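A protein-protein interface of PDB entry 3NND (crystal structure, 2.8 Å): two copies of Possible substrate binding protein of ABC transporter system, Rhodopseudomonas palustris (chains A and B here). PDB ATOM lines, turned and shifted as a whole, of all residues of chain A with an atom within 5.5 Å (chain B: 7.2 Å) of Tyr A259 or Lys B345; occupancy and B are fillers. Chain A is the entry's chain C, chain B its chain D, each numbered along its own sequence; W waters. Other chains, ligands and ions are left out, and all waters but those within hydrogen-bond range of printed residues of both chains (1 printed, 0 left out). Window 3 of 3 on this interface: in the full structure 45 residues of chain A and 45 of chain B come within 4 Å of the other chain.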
ATOM      1  N   TYR A 257      23.256  13.171  -4.052  1.00  0.00           N
ATOM      2  CA  TYR A 257      23.429  14.580  -3.712  1.00  0.00           C
ATOM      3  C   TYR A 257      22.512  15.464  -4.542  1.00  0.00           C
ATOM      4  O   TYR A 257      22.238  15.170  -5.696  1.00  0.00           O
ATOM      5  CB  TYR A 257      24.880  15.019  -3.922  1.00  0.00           C
ATOM      6  CG  TYR A 257      25.897  14.328  -3.037  1.00  0.00           C
ATOM      7  CD1 TYR A 257      26.241  14.855  -1.796  1.00  0.00           C
ATOM      8  CD2 TYR A 257      26.532  13.163  -3.451  1.00  0.00           C
ATOM      9  CE1 TYR A 257      27.172  14.231  -0.987  1.00  0.00           C
ATOM     10  CE2 TYR A 257      27.470  12.535  -2.651  1.00  0.00           C
ATOM     11  CZ  TYR A 257      27.783  13.075  -1.424  1.00  0.00           C
ATOM     12  OH  TYR A 257      28.710  12.459  -0.626  1.00  0.00           O
ATOM     13  N   TYR A 258      22.023  16.539  -3.947  1.00  0.00           N
ATOM     14  CA  TYR A 258      21.338  17.558  -4.717  1.00  0.00           C
ATOM     15  C   TYR A 258      22.280  18.739  -4.848  1.00  0.00           C
ATOM     16  O   TYR A 258      22.729  19.284  -3.838  1.00  0.00           O
ATOM     17  CB  TYR A 258      20.052  17.996  -4.026  1.00  0.00           C
ATOM     18  CG  TYR A 258      19.539  19.337  -4.504  1.00  0.00           C
ATOM     19  CD1 TYR A 258      18.543  19.422  -5.477  1.00  0.00           C
ATOM     20  CD2 TYR A 258      20.057  20.520  -3.993  1.00  0.00           C
ATOM     21  CE1 TYR A 258      18.071  20.650  -5.919  1.00  0.00           C
ATOM     22  CE2 TYR A 258      19.597  21.752  -4.429  1.00  0.00           C
ATOM     23  CZ  TYR A 258      18.606  21.814  -5.390  1.00  0.00           C
ATOM     24  OH  TYR A 258      18.158  23.043  -5.810  1.00  0.00           O
ATOM     25  N   TYR A 259      22.588  19.137  -6.079  1.00  0.00           N
ATOM     26  CA  TYR A 259      23.537  20.227  -6.281  1.00  0.00           C
ATOM     27  C   TYR A 259      22.853  21.556  -6.577  1.00  0.00           C
ATOM     28  O   TYR A 259      21.764  21.598  -7.139  1.00  0.00           O
ATOM     29  CB  TYR A 259      24.517  19.893  -7.397  1.00  0.00           C
ATOM     30  CG  TYR A 259      25.304  18.618  -7.191  1.00  0.00           C
ATOM     31  CD1 TYR A 259      26.580  18.640  -6.621  1.00  0.00           C
ATOM     32  CD2 TYR A 259      24.788  17.397  -7.589  1.00  0.00           C
ATOM     33  CE1 TYR A 259      27.311  17.465  -6.447  1.00  0.00           C
ATOM     34  CE2 TYR A 259      25.506  16.230  -7.419  1.00  0.00           C
ATOM     35  CZ  TYR A 259      26.761  16.267  -6.850  1.00  0.00           C
ATOM     36  OH  TYR A 259      27.440  15.086  -6.688  1.00  0.00           O
ATOM     37  N   TYR A 260      23.506  22.645  -6.192  1.00  0.00           N
ATOM     38  CA  TYR A 260      22.947  23.975  -6.387  1.00  0.00           C
ATOM     39  C   TYR A 260      24.008  25.071  -6.244  1.00  0.00           C
ATOM     40  O   TYR A 260      25.036  24.872  -5.596  1.00  0.00           O
ATOM     41  CB  TYR A 260      21.789  24.215  -5.418  1.00  0.00           C
ATOM     42  CG  TYR A 260      22.200  24.350  -3.975  1.00  0.00           C
ATOM     43  CD1 TYR A 260      22.281  25.595  -3.370  1.00  0.00           C
ATOM     44  CD2 TYR A 260      22.490  23.232  -3.210  1.00  0.00           C
ATOM     45  CE1 TYR A 260      22.646  25.718  -2.045  1.00  0.00           C
ATOM     46  CE2 TYR A 260      22.854  23.345  -1.885  1.00  0.00           C
ATOM     47  CZ  TYR A 260      22.929  24.589  -1.309  1.00  0.00           C
ATOM     48  OH  TYR A 260      23.296  24.704   0.015  1.00  0.00           O
ATOM     49  N   ASP A 261      23.755  26.231  -6.843  1.00  0.00           N
ATOM     50  CA  ASP A 261      24.763  27.275  -6.878  1.00  0.00           C
ATOM     51  C   ASP A 261      24.325  28.571  -6.226  1.00  0.00           C
ATOM     52  O   ASP A 261      23.213  29.037  -6.448  1.00  0.00           O
ATOM     53  CB  ASP A 261      25.206  27.536  -8.315  1.00  0.00           C
ATOM     54  CG  ASP A 261      25.965  26.368  -8.910  1.00  0.00           C
ATOM     55  OD1 ASP A 261      26.615  25.616  -8.151  1.00  0.00           O
ATOM     56  OD2 ASP A 261      25.906  26.199 -10.143  1.00  0.00           O
ATOM     57  N   PRO A 282      34.358  21.179   0.909  1.00  0.00           N
ATOM     58  CA  PRO A 282      33.618  22.440   0.852  1.00  0.00           C
ATOM     59  C   PRO A 282      32.503  22.441   1.879  1.00  0.00           C
ATOM     60  O   PRO A 282      32.069  21.377   2.298  1.00  0.00           O
ATOM     61  CB  PRO A 282      33.003  22.397  -0.543  1.00  0.00           C
ATOM     62  CG  PRO A 282      32.752  20.940  -0.736  1.00  0.00           C
ATOM     63  CD  PRO A 282      34.013  20.310  -0.228  1.00  0.00           C
ATOM     64  N   PRO A 283      32.031  23.631   2.267  1.00  0.00           N
ATOM     65  CA  PRO A 283      30.894  23.715   3.185  1.00  0.00           C
ATOM     66  C   PRO A 283      29.668  23.139   2.497  1.00  0.00           C
ATOM     67  O   PRO A 283      29.471  23.405   1.308  1.00  0.00           O
ATOM     68  CB  PRO A 283      30.693  25.225   3.368  1.00  0.00           C
ATOM     69  CG  PRO A 283      31.840  25.888   2.695  1.00  0.00           C
ATOM     70  CD  PRO A 283      32.383  24.938   1.692  1.00  0.00           C
ATOM     71  N   ASP A 284      28.850  22.372   3.209  1.00  0.00           N
ATOM     72  CA  ASP A 284      27.609  21.887   2.615  1.00  0.00           C
ATOM     73  C   ASP A 284      26.414  22.723   3.085  1.00  0.00           C
ATOM     74  O   ASP A 284      26.572  23.698   3.831  1.00  0.00           O
ATOM     75  CB  ASP A 284      27.415  20.380   2.874  1.00  0.00           C
ATOM     76  CG  ASP A 284      26.456  20.073   4.033  1.00  0.00           C
ATOM     77  OD1 ASP A 284      25.783  19.015   3.957  1.00  0.00           O
ATOM     78  OD2 ASP A 284      26.367  20.867   5.001  1.00  0.00           O
ATOM     79  N   PHE A 285      25.228  22.338   2.628  1.00  0.00           N
ATOM     80  CA  PHE A 285      23.980  23.004   2.984  1.00  0.00           C
ATOM     81  C   PHE A 285      23.797  23.160   4.495  1.00  0.00           C
ATOM     82  O   PHE A 285      23.426  24.226   4.988  1.00  0.00           O
ATOM     83  CB  PHE A 285      22.803  22.224   2.387  1.00  0.00           C
ATOM     84  CG  PHE A 285      21.463  22.741   2.794  1.00  0.00           C
ATOM     85  CD1 PHE A 285      21.002  23.952   2.311  1.00  0.00           C
ATOM     86  CD2 PHE A 285      20.658  22.010   3.657  1.00  0.00           C
ATOM     87  CE1 PHE A 285      19.766  24.432   2.686  1.00  0.00           C
ATOM     88  CE2 PHE A 285      19.414  22.483   4.040  1.00  0.00           C
ATOM     89  CZ  PHE A 285      18.966  23.694   3.554  1.00  0.00           C
ATOM     90  N   HIS B 343      29.535  26.532  -5.456  1.00  0.00           N
ATOM     91  CA  HIS B 343      28.703  25.353  -5.571  1.00  0.00           C
ATOM     92  C   HIS B 343      28.517  24.697  -4.213  1.00  0.00           C
ATOM     93  O   HIS B 343      29.477  24.441  -3.490  1.00  0.00           O
ATOM     94  CB  HIS B 343      29.301  24.390  -6.583  1.00  0.00           C
ATOM     95  CG  HIS B 343      29.815  25.072  -7.809  1.00  0.00           C
ATOM     96  ND1 HIS B 343      29.057  25.969  -8.529  1.00  0.00           N
ATOM     97  CD2 HIS B 343      31.017  25.010  -8.429  1.00  0.00           C
ATOM     98  CE1 HIS B 343      29.766  26.424  -9.548  1.00  0.00           C
ATOM     99  NE2 HIS B 343      30.960  25.857  -9.511  1.00  0.00           N
ATOM    100  N   PHE B 344      27.260  24.459  -3.867  1.00  0.00           N
ATOM    101  CA  PHE B 344      26.910  23.831  -2.610  1.00  0.00           C
ATOM    102  C   PHE B 344      26.065  22.632  -2.939  1.00  0.00           C
ATOM    103  O   PHE B 344      25.378  22.619  -3.953  1.00  0.00           O
ATOM    104  CB  PHE B 344      26.109  24.791  -1.742  1.00  0.00           C
ATOM    105  CG  PHE B 344      26.928  25.893  -1.141  1.00  0.00           C
ATOM    106  CD1 PHE B 344      27.329  25.830   0.184  1.00  0.00           C
ATOM    107  CD2 PHE B 344      27.294  26.990  -1.895  1.00  0.00           C
ATOM    108  CE1 PHE B 344      28.080  26.848   0.739  1.00  0.00           C
ATOM    109  CE2 PHE B 344      28.043  28.007  -1.346  1.00  0.00           C
ATOM    110  CZ  PHE B 344      28.435  27.942  -0.034  1.00  0.00           C
ATOM    111  N   LYS B 345      26.127  21.617  -2.093  1.00  0.00           N
ATOM    112  CA  LYS B 345      25.346  20.416  -2.304  1.00  0.00           C
ATOM    113  C   LYS B 345      24.805  19.939  -0.976  1.00  0.00           C
ATOM    114  O   LYS B 345      25.318  20.313   0.088  1.00  0.00           O
ATOM    115  CB  LYS B 345      26.203  19.318  -2.942  1.00  0.00           C
ATOM    116  CG  LYS B 345      27.286  18.744  -2.039  1.00  0.00           C
ATOM    117  CD  LYS B 345      28.080  17.659  -2.758  1.00  0.00           C
ATOM    118  CE  LYS B 345      29.434  17.409  -2.097  1.00  0.00           C
ATOM    119  NZ  LYS B 345      30.377  16.676  -2.994  1.00  0.00           N
ATOM    120  N   VAL B 346      23.764  19.118  -1.039  1.00  0.00           N
ATOM    121  CA  VAL B 346      23.261  18.439   0.148  1.00  0.00           C
ATOM    122  C   VAL B 346      23.130  16.936  -0.092  1.00  0.00           C
ATOM    123  O   VAL B 346      22.771  16.495  -1.188  1.00  0.00           O
ATOM    124  CB  VAL B 346      21.922  19.019   0.621  1.00  0.00           C
ATOM    125  CG1 VAL B 346      20.806  18.732  -0.387  1.00  0.00           C
ATOM    126  CG2 VAL B 346      21.578  18.460   1.983  1.00  0.00           C
ATOM    127  N   LYS B 347      23.447  16.158   0.937  1.00  0.00           N
ATOM    128  CA  LYS B 347      23.345  14.703   0.871  1.00  0.00           C
ATOM    129  C   LYS B 347      22.017  14.317   1.501  1.00  0.00           C
ATOM    130  O   LYS B 347      21.723  14.730   2.612  1.00  0.00           O
ATOM    131  CB  LYS B 347      24.530  14.082   1.609  1.00  0.00           C
ATOM    132  CG  LYS B 347      24.523  12.583   1.790  1.00  0.00           C
ATOM    133  CD  LYS B 347      25.971  12.123   1.967  1.00  0.00           C
ATOM    134  CE  LYS B 347      26.154  11.099   3.084  1.00  0.00           C
ATOM    135  NZ  LYS B 347      27.600  10.925   3.442  1.00  0.00           N
HETATM  136  O   HOH W   1      29.030  21.810  -0.906  1.00  0.00           O
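Water W1 lies within hydrogen-bond range of O of Pro A283 (2.8 Å) and N of Lys B345 (3.1 Å).
Tyr A259 touches just these residues of chain B: Phe B344 (3.8 Å) and Lys B345 (3.8 Å).
Of the printed residues of chain B, Asp A261 touches His B343.
Pro A282 touches none of the printed residues of chain B.
Of the printed residues of chain B, Asp A284 touches Lys B345.
Of the printed residues of chain A, His B343 touches Tyr A260 and Asp A261.
Lys B345 touches just these residues of chain A: Tyr A257, Tyr A258, Tyr A259, Tyr A260, Asp A284 and Phe A285.
The nearest residue of chain B that does not touch Tyr A259 is Val B346 (5.2 Å).
The nearest residue of chain A that does not touch Lys B345 is Pro A282 (5.0 Å).
The nearest printed residue of chain B that does not touch Pro A283 is His B343 (4.9 Å).
The backbone NH (N) of Tyr A258 is in hydrogen-bond range of the backbone carbonyl oxygen (O) of Val B346 (2.9 Å).
The backbone carbonyl oxygen (O) of Tyr A260 lies within hydrogen-bond range of the backbone NH (N) of Phe B344 (2.8 Å).
A ring nitrogen (ND1) of His B343 sits at hydrogen-bond distance from the side-chain carboxylate of Asp A261 (2.5 Å).
N of Phe A285 is in hydrogen-bond range of O of Lys B345, 3.2 Å away.
No position is printed for both chains.
Of the 15 pairs that touch across the chains among the printed residues, none has its exchanged pair printed and touching as well.
Among the printed residues, pairs that only touch across the chains: Tyr A257 with Val B346, Tyr A258 with Lys B345, Pro A283 with Phe B344, Asp A284 with Lys B345, Tyr A257 with Lys B345, Tyr A260 with His B343, Tyr A257 with Lys B347, Tyr A260 with Lys B345, Tyr A259 with Lys B345, Phe A285 with Val B346 and Tyr A259 with Phe B344.
Of the 9 printed residues of chain A, 8 touch a printed residue of chain B.
Among the printed residues, 15 pairs touch across the chains.
Among the printed residues, no Asp or Glu carboxylate lies within 4 Å of a Lys or Arg side-chain nitrogen of the other chain.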
